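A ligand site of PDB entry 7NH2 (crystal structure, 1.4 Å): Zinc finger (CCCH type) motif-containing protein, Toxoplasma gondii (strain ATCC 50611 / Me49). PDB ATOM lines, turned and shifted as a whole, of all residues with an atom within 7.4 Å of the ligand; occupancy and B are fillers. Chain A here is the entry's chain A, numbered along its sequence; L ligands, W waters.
OD2 of Asp 131 lies within hydrogen-bond range of OG1 of Thr 38, 3.0 Å away. The side-chain hydroxyl of Ser 21 sits close to the side-chain amide nitrogen of Asn 26. The side-chain hydroxyl (OG1) of Thr 38 sits close to the side-chain amide nitrogen (ND2) of Asn 42, at 3.5 Å. N of Asn 42 is in hydrogen-bond range of OG of Ser 39 (3.1 Å). The side-chain carboxylate (OD2) of Asp 131 is in hydrogen-bond range of the side-chain amide nitrogen (ND2) of Asn 42 (3.0 Å). The backbone NH of Lys 20 lies within hydrogen-bond range of the side-chain carboxylate of Asp 131. The side-chain amide oxygen of Asn 97 is in hydrogen-bond range of the indole nitrogen of Trp 87, 2.7 Å away.
Water W4 bridges NH1 of Arg 93 (2.6 Å) and N1 of the ligand (2.8 Å). Water W1 bridges OD1 of Asn 26 (2.7 Å) and N5 of the ligand (2.9 Å). Water W2 lies within hydrogen-bond range of OD1 of Asp 131 (2.7 Å), NE1 of Trp 36 (2.8 Å), OG1 of Thr 38 (2.9 Å) and N3 of the ligand (3.0 Å). Water W3 lies within hydrogen-bond range of the backbone carbonyl oxygen (O) of Lys 20 (2.7 Å), a nitrogen (N3) of the ligand (3.4 Å) and the side-chain amide nitrogen (ND2) of Asn 22 (3.4 Å).
Asn 26 touches the ligand (ND2 to N5, 3.8 Å). CZ2 of Trp 36 touches N4 of the ligand, 3.5 Å away. CA of Thr 38 touches N3 of the ligand, 3.6 Å away. Ser 39 touches the ligand. Trp 87 touches the ligand. Val 90 touches the ligand. CD2 of Leu 94 touches C3 of the ligand, at 3.5 Å. Asp 131 touches the ligand (OD2 to C2, 3.3 Å). Hydrophobic or aromatic side chains that line the ligand: Trp 36, Trp 87, Val 90 and Leu 94. Ten residues have an atom within 4 Å of the ligand: Asn 22, Asn 26, Trp 36, Ala 37, Thr 38, Ser 39, Trp 87, Val 90, Leu 94 and Asp 131. The nearest printed residue that does not touch the ligand is Arg 93 (4.5 Å).
A nitrogen (N1) of the ligand sits at hydrogen-bond distance from the side-chain amide nitrogen (ND2) of Asn 22. The backbone carbonyl oxygen (O) of Ala 37 sits at hydrogen-bond distance from a nitrogen (N4) of the ligand (2.8 Å).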
ATOM      1  N   ILE A  19     -25.348  26.207  13.196  1.00  0.00           N
ATOM      2  CA  ILE A  19     -25.735  24.929  12.606  1.00  0.00           C
ATOM      3  C   ILE A  19     -24.465  24.162  12.280  1.00  0.00           C
ATOM      4  O   ILE A  19     -23.561  24.694  11.637  1.00  0.00           O
ATOM      5  CB  ILE A  19     -26.548  25.172  11.325  1.00  0.00           C
ATOM      6  CG1 ILE A  19     -27.898  25.815  11.672  1.00  0.00           C
ATOM      7  CG2 ILE A  19     -26.685  23.868  10.536  1.00  0.00           C
ATOM      8  CD1 ILE A  19     -28.810  24.930  12.513  1.00  0.00           C
ATOM      9  N   LYS A  20     -24.396  22.933  12.769  1.00  0.00           N
ATOM     10  CA  LYS A  20     -23.272  22.075  12.439  1.00  0.00           C
ATOM     11  C   LYS A  20     -23.688  21.108  11.336  1.00  0.00           C
ATOM     12  O   LYS A  20     -24.810  20.599  11.316  1.00  0.00           O
ATOM     13  CB  LYS A  20     -22.786  21.288  13.658  1.00  0.00           C
ATOM     14  CG  LYS A  20     -22.262  22.147  14.801  1.00  0.00           C
ATOM     15  CD  LYS A  20     -21.104  23.058  14.389  1.00  0.00           C
ATOM     16  CE  LYS A  20     -19.817  22.260  14.139  1.00  0.00           C
ATOM     17  NZ  LYS A  20     -18.607  23.128  14.070  1.00  0.00           N
ATOM     18  N   SER A  21     -22.753  20.837  10.428  1.00  0.00           N
ATOM     19  CA  SER A  21     -22.973  19.879   9.354  1.00  0.00           C
ATOM     20  C   SER A  21     -21.921  18.789   9.471  1.00  0.00           C
ATOM     21  O   SER A  21     -20.725  19.092   9.589  1.00  0.00           O
ATOM     22  CB  SER A  21     -22.811  20.602   8.035  1.00  0.00           C
ATOM     23  OG  SER A  21     -22.944  19.679   6.969  1.00  0.00           O
ATOM     24  N   ASN A  22     -22.355  17.533   9.453  1.00  0.00           N
ATOM     25  CA  ASN A  22     -21.413  16.429   9.619  1.00  0.00           C
ATOM     26  C   ASN A  22     -20.778  15.972   8.315  1.00  0.00           C
ATOM     27  O   ASN A  22     -19.737  15.308   8.346  1.00  0.00           O
ATOM     28  CB  ASN A  22     -22.114  15.211  10.224  1.00  0.00           C
ATOM     29  CG  ASN A  22     -22.882  15.522  11.474  1.00  0.00           C
ATOM     30  OD1 ASN A  22     -22.312  15.783  12.535  1.00  0.00           O
ATOM     31  ND2 ASN A  22     -24.210  15.484  11.377  1.00  0.00           N
ATOM     32  N   ARG A  23     -21.395  16.271   7.179  1.00  0.00           N
ATOM     33  CA  ARG A  23     -20.833  15.913   5.878  1.00  0.00           C
ATOM     34  C   ARG A  23     -20.941  17.123   4.965  1.00  0.00           C
ATOM     35  O   ARG A  23     -21.953  17.822   4.983  1.00  0.00           O
ATOM     36  CB  ARG A  23     -21.514  14.658   5.250  1.00  0.00           C
ATOM     37  CG  ARG A  23     -22.997  14.555   5.490  1.00  0.00           C
ATOM     38  CD  ARG A  23     -23.641  13.197   5.100  1.00  0.00           C
ATOM     39  NE  ARG A  23     -22.984  12.499   3.991  1.00  0.00           N
ATOM     40  CZ  ARG A  23     -23.224  11.237   3.622  1.00  0.00           C
ATOM     41  NH1 ARG A  23     -24.117  10.488   4.260  1.00  0.00           N
ATOM     42  NH2 ARG A  23     -22.579  10.736   2.598  1.00  0.00           N
ATOM     43  N   ASN A  26     -24.011  17.824   2.792  1.00  0.00           N
ATOM     44  CA  ASN A  26     -25.174  18.512   3.356  1.00  0.00           C
ATOM     45  C   ASN A  26     -25.170  19.974   2.950  1.00  0.00           C
ATOM     46  O   ASN A  26     -26.194  20.534   2.557  1.00  0.00           O
ATOM     47  CB  ASN A  26     -25.137  18.444   4.894  1.00  0.00           C
ATOM     48  CG  ASN A  26     -25.259  17.041   5.439  1.00  0.00           C
ATOM     49  OD1 ASN A  26     -25.712  16.128   4.747  1.00  0.00           O
ATOM     50  ND2 ASN A  26     -24.869  16.879   6.690  1.00  0.00           N
ATOM     51  N   ILE A  27     -24.009  20.613   3.070  1.00  0.00           N
ATOM     52  CA  ILE A  27     -23.894  22.016   2.720  1.00  0.00           C
ATOM     53  C   ILE A  27     -24.105  22.225   1.228  1.00  0.00           C
ATOM     54  O   ILE A  27     -24.803  23.150   0.806  1.00  0.00           O
ATOM     55  CB  ILE A  27     -22.544  22.550   3.225  1.00  0.00           C
ATOM     56  CG1 ILE A  27     -22.601  22.758   4.737  1.00  0.00           C
ATOM     57  CG2 ILE A  27     -22.196  23.847   2.537  1.00  0.00           C
ATOM     58  CD1 ILE A  27     -21.270  23.129   5.350  1.00  0.00           C
ATOM     59  N   SER A  30     -27.706  21.914   0.531  1.00  0.00           N
ATOM     60  CA  SER A  30     -28.439  23.033   1.106  1.00  0.00           C
ATOM     61  C   SER A  30     -28.314  24.268   0.216  1.00  0.00           C
ATOM     62  O   SER A  30     -29.290  24.987  -0.015  1.00  0.00           O
ATOM     63  CB  SER A  30     -27.893  23.322   2.511  1.00  0.00           C
ATOM     64  OG  SER A  30     -28.526  24.455   3.060  1.00  0.00           O
ATOM     65  N   VAL A  35     -32.352  24.611   1.279  1.00  0.00           N
ATOM     66  CA  VAL A  35     -33.081  23.721   2.169  1.00  0.00           C
ATOM     67  C   VAL A  35     -32.175  23.302   3.312  1.00  0.00           C
ATOM     68  O   VAL A  35     -30.955  23.198   3.148  1.00  0.00           O
ATOM     69  CB  VAL A  35     -33.606  22.504   1.375  1.00  0.00           C
ATOM     70  CG1 VAL A  35     -32.457  21.683   0.799  1.00  0.00           C
ATOM     71  CG2 VAL A  35     -34.525  21.653   2.262  1.00  0.00           C
ATOM     72  N   TRP A  36     -32.776  23.052   4.473  1.00  0.00           N
ATOM     73  CA  TRP A  36     -32.056  22.478   5.602  1.00  0.00           C
ATOM     74  C   TRP A  36     -33.016  21.584   6.390  1.00  0.00           C
ATOM     75  O   TRP A  36     -34.229  21.634   6.210  1.00  0.00           O
ATOM     76  CB  TRP A  36     -31.435  23.562   6.508  1.00  0.00           C
ATOM     77  CG  TRP A  36     -30.407  22.987   7.460  1.00  0.00           C
ATOM     78  CD1 TRP A  36     -30.482  22.929   8.825  1.00  0.00           C
ATOM     79  CD2 TRP A  36     -29.175  22.350   7.104  1.00  0.00           C
ATOM     80  NE1 TRP A  36     -29.364  22.307   9.338  1.00  0.00           N
ATOM     81  CE2 TRP A  36     -28.546  21.943   8.308  1.00  0.00           C
ATOM     82  CE3 TRP A  36     -28.528  22.108   5.882  1.00  0.00           C
ATOM     83  CZ2 TRP A  36     -27.310  21.298   8.318  1.00  0.00           C
ATOM     84  CZ3 TRP A  36     -27.306  21.465   5.895  1.00  0.00           C
ATOM     85  CH2 TRP A  36     -26.711  21.070   7.106  1.00  0.00           C
ATOM     86  N   ALA A  37     -32.439  20.745   7.250  1.00  0.00           N
ATOM     87  CA  ALA A  37     -33.192  20.043   8.277  1.00  0.00           C
ATOM     88  C   ALA A  37     -32.262  19.832   9.459  1.00  0.00           C
ATOM     89  O   ALA A  37     -31.035  19.820   9.304  1.00  0.00           O
ATOM     90  CB  ALA A  37     -33.757  18.700   7.794  1.00  0.00           C
ATOM     91  N   THR A  38     -32.841  19.691  10.649  1.00  0.00           N
ATOM     92  CA  THR A  38     -32.060  19.517  11.861  1.00  0.00           C
ATOM     93  C   THR A  38     -32.728  18.440  12.720  1.00  0.00           C
ATOM     94  O   THR A  38     -33.753  17.871  12.339  1.00  0.00           O
ATOM     95  CB  THR A  38     -31.837  20.863  12.568  1.00  0.00           C
ATOM     96  OG1 THR A  38     -30.951  20.702  13.672  1.00  0.00           O
ATOM     97  CG2 THR A  38     -33.162  21.471  13.040  1.00  0.00           C
ATOM     98  N   SER A  39     -32.119  18.155  13.879  1.00  0.00           N
ATOM     99  CA  SER A  39     -32.685  17.185  14.804  1.00  0.00           C
ATOM    100  C   SER A  39     -34.092  17.609  15.219  1.00  0.00           C
ATOM    101  O   SER A  39     -34.476  18.774  15.105  1.00  0.00           O
ATOM    102  CB  SER A  39     -31.818  17.087  16.060  1.00  0.00           C
ATOM    103  OG  SER A  39     -31.980  18.269  16.828  1.00  0.00           O
ATOM    104  N   LYS A  40     -34.851  16.645  15.739  1.00  0.00           N
ATOM    105  CA  LYS A  40     -36.228  16.938  16.104  1.00  0.00           C
ATOM    106  C   LYS A  40     -36.303  17.994  17.200  1.00  0.00           C
ATOM    107  O   LYS A  40     -37.159  18.895  17.151  1.00  0.00           O
ATOM    108  CB  LYS A  40     -36.962  15.650  16.483  1.00  0.00           C
ATOM    109  CG  LYS A  40     -37.491  14.906  15.261  1.00  0.00           C
ATOM    110  CD  LYS A  40     -37.624  13.413  15.512  1.00  0.00           C
ATOM    111  CE  LYS A  40     -37.674  12.632  14.202  1.00  0.00           C
ATOM    112  NZ  LYS A  40     -38.709  11.553  14.207  1.00  0.00           N
ATOM    113  N   ASN A  42     -33.985  20.408  17.818  1.00  0.00           N
ATOM    114  CA  ASN A  42     -33.613  21.685  17.236  1.00  0.00           C
ATOM    115  C   ASN A  42     -34.675  22.189  16.272  1.00  0.00           C
ATOM    116  O   ASN A  42     -34.816  23.404  16.100  1.00  0.00           O
ATOM    117  CB  ASN A  42     -32.277  21.571  16.509  1.00  0.00           C
ATOM    118  CG  ASN A  42     -31.096  21.611  17.439  1.00  0.00           C
ATOM    119  OD1 ASN A  42     -31.203  22.043  18.586  1.00  0.00           O
ATOM    120  ND2 ASN A  42     -29.944  21.185  16.946  1.00  0.00           N
ATOM    121  N   ILE A  86     -34.450  14.177   0.805  1.00  0.00           N
ATOM    122  CA  ILE A  86     -33.328  14.679  -0.002  1.00  0.00           C
ATOM    123  C   ILE A  86     -31.975  14.328   0.610  1.00  0.00           C
ATOM    124  O   ILE A  86     -30.986  14.176  -0.110  1.00  0.00           O
ATOM    125  CB  ILE A  86     -33.482  16.191  -0.252  1.00  0.00           C
ATOM    126  CG1 ILE A  86     -32.457  16.677  -1.289  1.00  0.00           C
ATOM    127  CG2 ILE A  86     -33.369  17.004   1.061  1.00  0.00           C
ATOM    128  CD1 ILE A  86     -32.663  18.097  -1.734  1.00  0.00           C
ATOM    129  N   TRP A  87     -31.907  14.191   1.942  1.00  0.00           N
ATOM    130  CA  TRP A  87     -30.651  13.894   2.618  1.00  0.00           C
ATOM    131  C   TRP A  87     -30.334  12.402   2.638  1.00  0.00           C
ATOM    132  O   TRP A  87     -29.251  12.027   3.112  1.00  0.00           O
ATOM    133  CB  TRP A  87     -30.709  14.365   4.068  1.00  0.00           C
ATOM    134  CG  TRP A  87     -31.256  15.733   4.198  1.00  0.00           C
ATOM    135  CD1 TRP A  87     -32.490  16.066   4.675  1.00  0.00           C
ATOM    136  CD2 TRP A  87     -30.625  16.958   3.830  1.00  0.00           C
ATOM    137  NE1 TRP A  87     -32.668  17.416   4.616  1.00  0.00           N
ATOM    138  CE2 TRP A  87     -31.535  17.993   4.111  1.00  0.00           C
ATOM    139  CE3 TRP A  87     -29.366  17.279   3.307  1.00  0.00           C
ATOM    140  CZ2 TRP A  87     -31.233  19.327   3.875  1.00  0.00           C
ATOM    141  CZ3 TRP A  87     -29.073  18.607   3.071  1.00  0.00           C
ATOM    142  CH2 TRP A  87     -30.004  19.602   3.351  1.00  0.00           C
ATOM    143  N   VAL A  90     -30.772   9.402   6.548  1.00  0.00           N
ATOM    144  CA  VAL A  90     -30.695  10.231   7.737  1.00  0.00           C
ATOM    145  C   VAL A  90     -31.955  11.071   7.946  1.00  0.00           C
ATOM    146  O   VAL A  90     -32.245  11.477   9.071  1.00  0.00           O
ATOM    147  CB  VAL A  90     -29.409  11.073   7.744  1.00  0.00           C
ATOM    148  CG1 VAL A  90     -29.522  12.232   6.775  1.00  0.00           C
ATOM    149  CG2 VAL A  90     -29.093  11.573   9.151  1.00  0.00           C
ATOM    150  N   GLN A  91     -32.715  11.352   6.874  1.00  0.00           N
ATOM    151  CA  GLN A  91     -33.996  12.043   7.010  1.00  0.00           C
ATOM    152  C   GLN A  91     -34.859  11.412   8.094  1.00  0.00           C
ATOM    153  O   GLN A  91     -35.629  12.105   8.773  1.00  0.00           O
ATOM    154  CB  GLN A  91     -34.731  12.019   5.666  1.00  0.00           C
ATOM    155  CG  GLN A  91     -35.972  12.898   5.601  1.00  0.00           C
ATOM    156  CD  GLN A  91     -35.652  14.322   5.197  1.00  0.00           C
ATOM    157  OE1 GLN A  91     -35.293  14.581   4.059  1.00  0.00           O
ATOM    158  NE2 GLN A  91     -35.807  15.245   6.129  1.00  0.00           N
ATOM    159  N   ARG A  93     -34.097  10.369  10.993  1.00  0.00           N
ATOM    160  CA  ARG A  93     -33.823  10.851  12.344  1.00  0.00           C
ATOM    161  C   ARG A  93     -33.809  12.370  12.474  1.00  0.00           C
ATOM    162  O   ARG A  93     -33.360  12.891  13.492  1.00  0.00           O
ATOM    163  CB  ARG A  93     -32.564  10.220  12.954  1.00  0.00           C
ATOM    164  CG  ARG A  93     -31.331  10.157  12.067  1.00  0.00           C
ATOM    165  CD  ARG A  93     -30.190   9.505  12.838  1.00  0.00           C
ATOM    166  NE  ARG A  93     -28.996   9.268  12.041  1.00  0.00           N
ATOM    167  CZ  ARG A  93     -27.898  10.016  12.092  1.00  0.00           C
ATOM    168  NH1 ARG A  93     -27.837  11.056  12.918  1.00  0.00           N
ATOM    169  NH2 ARG A  93     -26.845   9.721  11.324  1.00  0.00           N
ATOM    170  N   LEU A  94     -34.287  13.089  11.461  1.00  0.00           N
ATOM    171  CA  LEU A  94     -34.359  14.543  11.497  1.00  0.00           C
ATOM    172  C   LEU A  94     -35.807  15.005  11.515  1.00  0.00           C
ATOM    173  O   LEU A  94     -36.738  14.212  11.308  1.00  0.00           O
ATOM    174  CB  LEU A  94     -33.634  15.142  10.290  1.00  0.00           C
ATOM    175  CG  LEU A  94     -32.176  14.698  10.119  1.00  0.00           C
ATOM    176  CD1 LEU A  94     -31.602  15.181   8.784  1.00  0.00           C
ATOM    177  CD2 LEU A  94     -31.331  15.192  11.290  1.00  0.00           C
ATOM    178  N   ASN A  97     -37.924  19.012   6.395  1.00  0.00           N
ATOM    179  CA  ASN A  97     -37.107  20.015   5.725  1.00  0.00           C
ATOM    180  C   ASN A  97     -37.777  21.383   5.745  1.00  0.00           C
ATOM    181  O   ASN A  97     -39.002  21.497   5.686  1.00  0.00           O
ATOM    182  CB  ASN A  97     -36.854  19.567   4.285  1.00  0.00           C
ATOM    183  CG  ASN A  97     -36.093  18.259   4.236  1.00  0.00           C
ATOM    184  OD1 ASN A  97     -35.300  17.973   5.107  1.00  0.00           O
ATOM    185  ND2 ASN A  97     -36.362  17.441   3.216  1.00  0.00           N
ATOM    186  N   ASP A 131     -24.639  21.717  17.358  1.00  0.00           N
ATOM    187  CA  ASP A 131     -25.692  22.059  16.415  1.00  0.00           C
ATOM    188  C   ASP A 131     -26.895  22.669  17.141  1.00  0.00           C
ATOM    189  O   ASP A 131     -27.359  22.114  18.154  1.00  0.00           O
ATOM    190  CB  ASP A 131     -26.118  20.768  15.709  1.00  0.00           C
ATOM    191  CG  ASP A 131     -27.180  20.990  14.663  1.00  0.00           C
ATOM    192  OD1 ASP A 131     -26.969  21.838  13.767  1.00  0.00           O
ATOM    193  OD2 ASP A 131     -28.220  20.296  14.720  1.00  0.00           O
ATOM    194  N   GLY A 132     -27.372  23.808  16.643  1.00  0.00           N
ATOM    195  CA  GLY A 132     -28.509  24.513  17.214  1.00  0.00           C
ATOM    196  C   GLY A 132     -28.198  25.473  18.345  1.00  0.00           C
ATOM    197  O   GLY A 132     -29.131  26.052  18.907  1.00  0.00           O
HETATM  198  N1  LIG L   1     -27.538  14.950  10.648  1.00  0.00           N
HETATM  199  C1  LIG L   1     -27.597  15.553  13.735  1.00  0.00           C
HETATM  200  C2  LIG L   1     -28.477  17.646  12.736  1.00  0.00           C
HETATM  201  C3  LIG L   1     -27.941  16.073  11.309  1.00  0.00           C
HETATM  202  C4  LIG L   1     -28.393  17.152  10.606  1.00  0.00           C
HETATM  203  C5  LIG L   1     -28.434  17.039   9.192  1.00  0.00           C
HETATM  204  C6  LIG L   1     -29.149  18.056   6.976  1.00  0.00           C
HETATM  205  C7  LIG L   1     -27.582  14.888   9.332  1.00  0.00           C
HETATM  206  N2  LIG L   1     -28.000  16.411  12.632  1.00  0.00           N
HETATM  207  N3  LIG L   1     -28.734  18.122  11.515  1.00  0.00           N
HETATM  208  N4  LIG L   1     -28.932  18.153   8.409  1.00  0.00           N
HETATM  209  N5  LIG L   1     -28.022  15.915   8.621  1.00  0.00           N
HETATM  210  O   HOH W   1     -27.551  14.620   6.062  1.00  0.00           O
HETATM  211  O   HOH W   2     -28.763  21.108  11.820  1.00  0.00           O
HETATM  212  O   HOH W   3     -25.562  18.363  12.648  1.00  0.00           O
HETATM  213  O   HOH W   4     -26.337  12.531  11.454  1.00  0.00           O
HETATM  214  O   HOH W   5     -26.813  13.661  16.049  1.00  0.00           O
HETATM  215  O   HOH W   6     -26.164  16.575  16.380  1.00  0.00           O
